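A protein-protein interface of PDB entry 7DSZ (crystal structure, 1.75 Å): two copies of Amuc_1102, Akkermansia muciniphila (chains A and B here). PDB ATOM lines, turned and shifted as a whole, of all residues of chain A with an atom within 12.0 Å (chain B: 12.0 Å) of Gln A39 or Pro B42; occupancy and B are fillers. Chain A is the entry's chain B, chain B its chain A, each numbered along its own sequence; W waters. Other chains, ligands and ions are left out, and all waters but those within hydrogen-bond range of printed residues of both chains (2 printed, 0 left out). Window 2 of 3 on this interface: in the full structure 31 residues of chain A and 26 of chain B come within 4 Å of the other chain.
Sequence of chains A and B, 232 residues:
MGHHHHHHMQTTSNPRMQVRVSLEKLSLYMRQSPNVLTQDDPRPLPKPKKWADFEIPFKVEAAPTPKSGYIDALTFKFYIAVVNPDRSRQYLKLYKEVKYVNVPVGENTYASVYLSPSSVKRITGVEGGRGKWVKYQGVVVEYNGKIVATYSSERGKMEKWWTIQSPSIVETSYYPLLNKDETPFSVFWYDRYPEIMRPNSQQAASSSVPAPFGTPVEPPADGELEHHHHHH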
ATOM      1  N   ASN A  35     -17.594  -3.211  10.723  1.00  0.00           N
ATOM      2  CA  ASN A  35     -17.966  -4.033  11.868  1.00  0.00           C
ATOM      3  C   ASN A  35     -17.573  -5.456  11.504  1.00  0.00           C
ATOM      4  O   ASN A  35     -18.274  -6.132  10.750  1.00  0.00           O
ATOM      5  CB  ASN A  35     -19.454  -3.915  12.181  1.00  0.00           C
ATOM      6  CG  ASN A  35     -19.747  -2.851  13.217  1.00  0.00           C
ATOM      7  OD1 ASN A  35     -18.916  -2.564  14.082  1.00  0.00           O
ATOM      8  ND2 ASN A  35     -20.933  -2.257  13.136  1.00  0.00           N
ATOM      9  N   VAL A  36     -16.421  -5.896  12.004  1.00  0.00           N
ATOM     10  CA  VAL A  36     -15.966  -7.256  11.747  1.00  0.00           C
ATOM     11  C   VAL A  36     -16.799  -8.223  12.575  1.00  0.00           C
ATOM     12  O   VAL A  36     -16.962  -8.042  13.788  1.00  0.00           O
ATOM     13  CB  VAL A  36     -14.472  -7.384  12.078  1.00  0.00           C
ATOM     14  CG1 VAL A  36     -14.050  -8.830  12.053  1.00  0.00           C
ATOM     15  CG2 VAL A  36     -13.638  -6.537  11.114  1.00  0.00           C
ATOM     16  N   LEU A  37     -17.306  -9.275  11.933  1.00  0.00           N
ATOM     17  CA  LEU A  37     -18.144 -10.255  12.624  1.00  0.00           C
ATOM     18  C   LEU A  37     -17.300 -11.282  13.366  1.00  0.00           C
ATOM     19  O   LEU A  37     -16.260 -11.724  12.869  1.00  0.00           O
ATOM     20  CB  LEU A  37     -19.053 -10.969  11.628  1.00  0.00           C
ATOM     21  CG  LEU A  37     -19.924 -10.027  10.808  1.00  0.00           C
ATOM     22  CD1 LEU A  37     -20.870 -10.828   9.933  1.00  0.00           C
ATOM     23  CD2 LEU A  37     -20.682  -9.099  11.735  1.00  0.00           C
ATOM     24  N   THR A  38     -17.774 -11.689  14.549  1.00  0.00           N
ATOM     25  CA  THR A  38     -17.089 -12.688  15.362  1.00  0.00           C
ATOM     26  C   THR A  38     -18.042 -13.822  15.722  1.00  0.00           C
ATOM     27  O   THR A  38     -19.266 -13.674  15.667  1.00  0.00           O
ATOM     28  CB  THR A  38     -16.501 -12.092  16.656  1.00  0.00           C
ATOM     29  OG1 THR A  38     -17.533 -11.418  17.386  1.00  0.00           O
ATOM     30  CG2 THR A  38     -15.373 -11.110  16.343  1.00  0.00           C
ATOM     31  N   GLN A  39     -17.452 -14.960  16.105  1.00  0.00           N
ATOM     32  CA  GLN A  39     -18.241 -16.154  16.417  1.00  0.00           C
ATOM     33  C   GLN A  39     -19.144 -15.921  17.621  1.00  0.00           C
ATOM     34  O   GLN A  39     -20.333 -16.260  17.597  1.00  0.00           O
ATOM     35  CB  GLN A  39     -17.309 -17.344  16.662  1.00  0.00           C
ATOM     36  CG  GLN A  39     -17.996 -18.707  16.633  1.00  0.00           C
ATOM     37  CD  GLN A  39     -17.176 -19.767  15.899  1.00  0.00           C
ATOM     38  OE1 GLN A  39     -16.752 -19.565  14.756  1.00  0.00           O
ATOM     39  NE2 GLN A  39     -16.948 -20.903  16.557  1.00  0.00           N
ATOM     40  N   ASP A  40     -18.594 -15.341  18.689  1.00  0.00           N
ATOM     41  CA  ASP A  40     -19.363 -15.018  19.892  1.00  0.00           C
ATOM     42  C   ASP A  40     -20.103 -13.688  19.715  1.00  0.00           C
ATOM     43  O   ASP A  40     -19.894 -12.721  20.449  1.00  0.00           O
ATOM     44  CB  ASP A  40     -18.448 -14.971  21.112  1.00  0.00           C
ATOM     45  CG  ASP A  40     -18.013 -16.354  21.582  1.00  0.00           C
ATOM     46  OD1 ASP A  40     -17.419 -17.104  20.775  1.00  0.00           O
ATOM     47  OD2 ASP A  40     -18.252 -16.682  22.766  1.00  0.00           O
ATOM     48  N   ASP A  41     -20.981 -13.658  18.712  1.00  0.00           N
ATOM     49  CA  ASP A  41     -21.782 -12.471  18.411  1.00  0.00           C
ATOM     50  C   ASP A  41     -20.898 -11.238  18.234  1.00  0.00           C
ATOM     51  O   ASP A  41     -20.875 -10.354  19.095  1.00  0.00           O
ATOM     52  CB  ASP A  41     -22.812 -12.228  19.521  1.00  0.00           C
ATOM     53  CG  ASP A  41     -23.864 -11.198  19.140  1.00  0.00           C
ATOM     54  OD1 ASP A  41     -23.570 -10.270  18.354  1.00  0.00           O
ATOM     55  OD2 ASP A  41     -25.000 -11.318  19.643  1.00  0.00           O
ATOM     56  N   LEU A  45     -23.878  -4.763  18.618  1.00  0.00           N
ATOM     57  CA  LEU A  45     -23.208  -4.230  17.432  1.00  0.00           C
ATOM     58  C   LEU A  45     -23.201  -2.701  17.450  1.00  0.00           C
ATOM     59  O   LEU A  45     -24.262  -2.074  17.420  1.00  0.00           O
ATOM     60  CB  LEU A  45     -23.888  -4.736  16.157  1.00  0.00           C
ATOM     61  CG  LEU A  45     -23.023  -4.786  14.893  1.00  0.00           C
ATOM     62  CD1 LEU A  45     -22.515  -6.205  14.634  1.00  0.00           C
ATOM     63  CD2 LEU A  45     -23.788  -4.247  13.692  1.00  0.00           C
ATOM     64  N   ARG B  31     -10.131 -11.919  29.138  1.00  0.00           N
ATOM     65  CA  ARG B  31     -11.041 -11.931  27.998  1.00  0.00           C
ATOM     66  C   ARG B  31     -10.516 -12.804  26.861  1.00  0.00           C
ATOM     67  O   ARG B  31      -9.312 -12.837  26.581  1.00  0.00           O
ATOM     68  CB  ARG B  31     -11.289 -10.496  27.479  1.00  0.00           C
ATOM     69  CG  ARG B  31     -11.915  -9.541  28.505  1.00  0.00           C
ATOM     70  CD  ARG B  31     -12.132  -8.186  27.890  1.00  0.00           C
ATOM     71  NE  ARG B  31     -12.811  -8.355  26.624  1.00  0.00           N
ATOM     72  CZ  ARG B  31     -12.607  -7.603  25.557  1.00  0.00           C
ATOM     73  NH1 ARG B  31     -11.729  -6.608  25.586  1.00  0.00           N
ATOM     74  NH2 ARG B  31     -13.282  -7.862  24.451  1.00  0.00           N
ATOM     75  N   GLN B  32     -11.436 -13.511  26.204  1.00  0.00           N
ATOM     76  CA  GLN B  32     -11.089 -14.236  24.994  1.00  0.00           C
ATOM     77  C   GLN B  32     -10.729 -13.245  23.896  1.00  0.00           C
ATOM     78  O   GLN B  32     -11.323 -12.174  23.793  1.00  0.00           O
ATOM     79  CB  GLN B  32     -12.257 -15.095  24.511  1.00  0.00           C
ATOM     80  CG  GLN B  32     -12.900 -15.989  25.549  1.00  0.00           C
ATOM     81  CD  GLN B  32     -13.652 -17.153  24.915  1.00  0.00           C
ATOM     82  OE1 GLN B  32     -13.131 -18.268  24.823  1.00  0.00           O
ATOM     83  NE2 GLN B  32     -14.877 -16.894  24.466  1.00  0.00           N
ATOM     84  N   SER B  33      -9.760 -13.609  23.069  1.00  0.00           N
ATOM     85  CA  SER B  33      -9.582 -12.863  21.838  1.00  0.00           C
ATOM     86  C   SER B  33     -10.828 -13.034  20.967  1.00  0.00           C
ATOM     87  O   SER B  33     -11.535 -14.041  21.072  1.00  0.00           O
ATOM     88  CB  SER B  33      -8.341 -13.343  21.093  1.00  0.00           C
ATOM     89  OG  SER B  33      -8.260 -14.750  21.110  1.00  0.00           O
ATOM     90  N   PRO B  34     -11.140 -12.056  20.122  1.00  0.00           N
ATOM     91  CA  PRO B  34     -12.270 -12.232  19.205  1.00  0.00           C
ATOM     92  C   PRO B  34     -12.007 -13.415  18.289  1.00  0.00           C
ATOM     93  O   PRO B  34     -10.889 -13.631  17.824  1.00  0.00           O
ATOM     94  CB  PRO B  34     -12.312 -10.911  18.430  1.00  0.00           C
ATOM     95  CG  PRO B  34     -11.563  -9.933  19.299  1.00  0.00           C
ATOM     96  CD  PRO B  34     -10.498 -10.742  19.962  1.00  0.00           C
ATOM     97  N   ASN B  35     -13.037 -14.220  18.077  1.00  0.00           N
ATOM     98  CA  ASN B  35     -12.952 -15.294  17.095  1.00  0.00           C
ATOM     99  C   ASN B  35     -13.547 -14.728  15.815  1.00  0.00           C
ATOM    100  O   ASN B  35     -14.758 -14.718  15.615  1.00  0.00           O
ATOM    101  CB  ASN B  35     -13.685 -16.539  17.576  1.00  0.00           C
ATOM    102  CG  ASN B  35     -13.014 -17.799  17.124  1.00  0.00           C
ATOM    103  OD1 ASN B  35     -13.646 -18.668  16.528  1.00  0.00           O
ATOM    104  ND2 ASN B  35     -11.715 -17.908  17.391  1.00  0.00           N
ATOM    105  N   VAL B  36     -12.677 -14.207  14.958  1.00  0.00           N
ATOM    106  CA  VAL B  36     -13.139 -13.464  13.797  1.00  0.00           C
ATOM    107  C   VAL B  36     -13.659 -14.447  12.759  1.00  0.00           C
ATOM    108  O   VAL B  36     -13.037 -15.485  12.496  1.00  0.00           O
ATOM    109  CB  VAL B  36     -12.009 -12.578  13.251  1.00  0.00           C
ATOM    110  CG1 VAL B  36     -12.370 -11.997  11.899  1.00  0.00           C
ATOM    111  CG2 VAL B  36     -11.717 -11.464  14.260  1.00  0.00           C
ATOM    112  N   LEU B  37     -14.833 -14.156  12.216  1.00  0.00           N
ATOM    113  CA  LEU B  37     -15.423 -15.001  11.191  1.00  0.00           C
ATOM    114  C   LEU B  37     -14.807 -14.663   9.848  1.00  0.00           C
ATOM    115  O   LEU B  37     -14.574 -13.495   9.536  1.00  0.00           O
ATOM    116  CB  LEU B  37     -16.936 -14.806  11.125  1.00  0.00           C
ATOM    117  CG  LEU B  37     -17.750 -15.183  12.362  1.00  0.00           C
ATOM    118  CD1 LEU B  37     -19.235 -14.917  12.130  1.00  0.00           C
ATOM    119  CD2 LEU B  37     -17.502 -16.637  12.706  1.00  0.00           C
ATOM    120  N   THR B  38     -14.533 -15.687   9.057  1.00  0.00           N
ATOM    121  CA  THR B  38     -14.013 -15.495   7.716  1.00  0.00           C
ATOM    122  C   THR B  38     -14.931 -16.171   6.707  1.00  0.00           C
ATOM    123  O   THR B  38     -15.831 -16.939   7.060  1.00  0.00           O
ATOM    124  CB  THR B  38     -12.597 -16.057   7.590  1.00  0.00           C
ATOM    125  OG1 THR B  38     -12.618 -17.442   7.953  1.00  0.00           O
ATOM    126  CG2 THR B  38     -11.636 -15.301   8.507  1.00  0.00           C
ATOM    127  N   GLN B  39     -14.682 -15.865   5.434  1.00  0.00           N
ATOM    128  CA  GLN B  39     -15.423 -16.500   4.351  1.00  0.00           C
ATOM    129  C   GLN B  39     -15.276 -18.013   4.402  1.00  0.00           C
ATOM    130  O   GLN B  39     -16.222 -18.749   4.099  1.00  0.00           O
ATOM    131  CB  GLN B  39     -14.938 -15.962   3.003  1.00  0.00           C
ATOM    132  CG  GLN B  39     -15.901 -16.188   1.851  1.00  0.00           C
ATOM    133  CD  GLN B  39     -17.072 -15.225   1.878  1.00  0.00           C
ATOM    134  OE1 GLN B  39     -16.893 -14.003   1.869  1.00  0.00           O
ATOM    135  NE2 GLN B  39     -18.282 -15.771   1.923  1.00  0.00           N
ATOM    136  N   ASP B  40     -14.103 -18.498   4.808  1.00  0.00           N
ATOM    137  CA  ASP B  40     -13.824 -19.926   4.728  1.00  0.00           C
ATOM    138  C   ASP B  40     -14.482 -20.698   5.866  1.00  0.00           C
ATOM    139  O   ASP B  40     -15.358 -21.534   5.624  1.00  0.00           O
ATOM    140  CB  ASP B  40     -12.313 -20.165   4.681  1.00  0.00           C
ATOM    141  CG  ASP B  40     -11.871 -20.723   3.344  1.00  0.00           C
ATOM    142  OD1 ASP B  40     -12.457 -21.742   2.913  1.00  0.00           O
ATOM    143  OD2 ASP B  40     -10.970 -20.135   2.708  1.00  0.00           O
ATOM    144  N   ASP B  41     -14.086 -20.452   7.110  1.00  0.00           N
ATOM    145  CA  ASP B  41     -14.770 -21.116   8.222  1.00  0.00           C
ATOM    146  C   ASP B  41     -15.429 -20.095   9.150  1.00  0.00           C
ATOM    147  O   ASP B  41     -14.736 -19.292   9.805  1.00  0.00           O
ATOM    148  CB  ASP B  41     -13.834 -22.078   8.974  1.00  0.00           C
ATOM    149  CG  ASP B  41     -12.930 -21.402   9.996  1.00  0.00           C
ATOM    150  OD1 ASP B  41     -12.352 -20.333   9.706  1.00  0.00           O
ATOM    151  OD2 ASP B  41     -12.784 -21.974  11.099  1.00  0.00           O
ATOM    152  N   PRO B  42     -16.766 -20.033   9.171  1.00  0.00           N
ATOM    153  CA  PRO B  42     -17.577 -19.201  10.067  1.00  0.00           C
ATOM    154  C   PRO B  42     -18.019 -19.960  11.324  1.00  0.00           C
ATOM    155  O   PRO B  42     -19.193 -19.902  11.691  1.00  0.00           O
ATOM    156  CB  PRO B  42     -18.780 -18.834   9.198  1.00  0.00           C
ATOM    157  CG  PRO B  42     -18.949 -20.027   8.305  1.00  0.00           C
ATOM    158  CD  PRO B  42     -17.572 -20.608   8.078  1.00  0.00           C
ATOM    159  N   PRO B 184      -5.251  -8.186  19.347  1.00  0.00           N
ATOM    160  CA  PRO B 184      -6.402  -8.497  18.476  1.00  0.00           C
ATOM    161  C   PRO B 184      -7.656  -7.720  18.816  1.00  0.00           C
ATOM    162  O   PRO B 184      -8.636  -7.834  18.076  1.00  0.00           O
ATOM    163  CB  PRO B 184      -6.630 -10.001  18.704  1.00  0.00           C
ATOM    164  CG  PRO B 184      -5.439 -10.498  19.378  1.00  0.00           C
ATOM    165  CD  PRO B 184      -4.793  -9.371  20.086  1.00  0.00           C
ATOM    166  N   PHE B 185      -7.675  -6.958  19.910  1.00  0.00           N
ATOM    167  CA  PHE B 185      -8.833  -6.132  20.219  1.00  0.00           C
ATOM    168  C   PHE B 185      -8.842  -4.816  19.459  1.00  0.00           C
ATOM    169  O   PHE B 185      -9.802  -4.060  19.601  1.00  0.00           O
ATOM    170  CB  PHE B 185      -8.894  -5.871  21.730  1.00  0.00           C
ATOM    171  CG  PHE B 185      -8.940  -7.137  22.526  1.00  0.00           C
ATOM    172  CD1 PHE B 185     -10.095  -7.899  22.571  1.00  0.00           C
ATOM    173  CD2 PHE B 185      -7.823  -7.588  23.188  1.00  0.00           C
ATOM    174  CE1 PHE B 185     -10.139  -9.082  23.286  1.00  0.00           C
ATOM    175  CE2 PHE B 185      -7.853  -8.756  23.897  1.00  0.00           C
ATOM    176  CZ  PHE B 185      -9.014  -9.519  23.941  1.00  0.00           C
ATOM    177  N   VAL B 187      -9.549  -3.474  16.528  1.00  0.00           N
ATOM    178  CA  VAL B 187     -10.651  -2.912  15.737  1.00  0.00           C
ATOM    179  C   VAL B 187     -12.001  -3.035  16.427  1.00  0.00           C
ATOM    180  O   VAL B 187     -13.020  -2.647  15.839  1.00  0.00           O
ATOM    181  CB  VAL B 187     -10.756  -3.551  14.335  1.00  0.00           C
ATOM    182  CG1 VAL B 187      -9.419  -3.443  13.601  1.00  0.00           C
ATOM    183  CG2 VAL B 187     -11.200  -5.006  14.434  1.00  0.00           C
ATOM    184  N   PHE B 188     -12.046  -3.531  17.656  1.00  0.00           N
ATOM    185  CA  PHE B 188     -13.303  -3.787  18.344  1.00  0.00           C
ATOM    186  C   PHE B 188     -13.500  -2.790  19.470  1.00  0.00           C
ATOM    187  O   PHE B 188     -12.542  -2.185  19.958  1.00  0.00           O
ATOM    188  CB  PHE B 188     -13.327  -5.218  18.887  1.00  0.00           C
ATOM    189  CG  PHE B 188     -13.272  -6.252  17.804  1.00  0.00           C
ATOM    190  CD1 PHE B 188     -14.419  -6.600  17.116  1.00  0.00           C
ATOM    191  CD2 PHE B 188     -12.070  -6.839  17.438  1.00  0.00           C
ATOM    192  CE1 PHE B 188     -14.383  -7.545  16.103  1.00  0.00           C
ATOM    193  CE2 PHE B 188     -12.027  -7.782  16.416  1.00  0.00           C
ATOM    194  CZ  PHE B 188     -13.188  -8.126  15.747  1.00  0.00           C
ATOM    195  N   TRP B 189     -14.763  -2.615  19.865  1.00  0.00           N
ATOM    196  CA  TRP B 189     -15.118  -1.708  20.961  1.00  0.00           C
ATOM    197  C   TRP B 189     -14.525  -0.324  20.725  1.00  0.00           C
ATOM    198  O   TRP B 189     -13.990   0.315  21.640  1.00  0.00           O
ATOM    199  CB  TRP B 189     -14.638  -2.261  22.310  1.00  0.00           C
ATOM    200  CG  TRP B 189     -15.318  -3.485  22.830  1.00  0.00           C
ATOM    201  CD1 TRP B 189     -16.262  -4.258  22.208  1.00  0.00           C
ATOM    202  CD2 TRP B 189     -15.109  -4.070  24.122  1.00  0.00           C
ATOM    203  NE1 TRP B 189     -16.646  -5.295  23.040  1.00  0.00           N
ATOM    204  CE2 TRP B 189     -15.956  -5.194  24.220  1.00  0.00           C
ATOM    205  CE3 TRP B 189     -14.284  -3.749  25.202  1.00  0.00           C
ATOM    206  CZ2 TRP B 189     -15.988  -6.014  25.358  1.00  0.00           C
ATOM    207  CZ3 TRP B 189     -14.323  -4.563  26.340  1.00  0.00           C
ATOM    208  CH2 TRP B 189     -15.166  -5.678  26.399  1.00  0.00           C
HETATM  209  O   HOH W   1     -15.103  -4.292  14.132  1.00  0.00           O
HETATM  210  O   HOH W   2     -15.289 -14.670  19.301  1.00  0.00           O
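Of the 8 printed residues of chain A, 5 touch a printed residue of chain B.
Printed residues of chain A that touch a printed residue of chain B: Val A36, Leu A37, Thr A38, Gln A39 and Asp A40.
Of the 17 printed residues of chain B, 7 touch a printed residue of chain A.
Hydrophobic or aromatic side chains of chain B that line the printed part of chain A: Pro B34, Val B36, Leu B37 and Phe B188.
Along chain B the printed residues that touch a printed residue of chain A span positions 32 to 188.
Among the printed residues, no Asp or Glu carboxylate lies within 4 Å of a Lys or Arg side-chain nitrogen of the other chain.
Among the printed residues, merely in contact across the chains: Val A36 with Val B36, Val A36 with Phe B188, Leu A37 with Val B36, Thr A38 with Pro B34, Thr A38 with Asn B35, Thr A38 with Leu B37, Thr A38 with Phe B188, Gln A39 with Leu B37, Gln A39 with Pro B42 and Asp A40 with Gln B32.
Leu A37 touches Val B36, but with the chains exchanged Val A36 does not touch Leu B37 (5.3 Å).
Leu B37 touches its own counterpart, Leu A37.
Gln A39 touches Asn B35, but with the chains exchanged Asn A35 does not touch Gln B39 (11.7 Å).
Gln A39 touches Leu B37, but with the chains exchanged Leu A37 does not touch Gln B39 (8.7 Å).
Water W2 bridges the backbone NH (N) of Asn B35 (2.6 Å) and the backbone NH (N) of Asp A40 (3.4 Å).
Water W1 lies within hydrogen-bond range of the backbone NH of Val A36 and the backbone carbonyl oxygen of Val B187.
Of chain B, only Asn B35 (2.7 Å), Leu B37 (3.7 Å) and Pro B42 (3.7 Å) come within 4 Å of Gln A39.
Pro B42 touches just one residue of chain A: Gln A39 (3.7 Å).
Asp A40 touches just one residue of chain B: Gln B32.
No residue of chain B comes within 4 Å of Asp A41.
Of chain A, only Thr A38 (3.1 Å) and Gln A39 (2.7 Å) come within 4 Å of Asn B35.
No residue of chain A comes within 4 Å of Thr B38.
No residue of chain A comes within 4 Å of Asp B41.
Printed residues of chain A within 4 Å of Gln B32: Asp A40 (3.8 Å).
Printed residues of chain B within 4 Å of Leu A37: Val B36 and Leu B37.
Printed residues of chain A within 4 Å of Pro B34: Thr A38 (3.7 Å).
Printed residues of chain B within 4 Å of Val A36: Val B36 and Phe B188.
Of the printed residues of chain A, Phe B188 touches Val A36 and Thr A38.
The nearest residue of chain B that does not touch Gln A39 is Val B36 (5.0 Å).
The nearest printed residue of chain A that does not touch Phe B188 is Leu A37 (5.4 Å).
O of Asn B35 sits at hydrogen-bond distance from N of Gln A39, 2.7 Å away.
N of Leu B37 lies within hydrogen-bond range of O of Leu A37 (2.9 Å).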
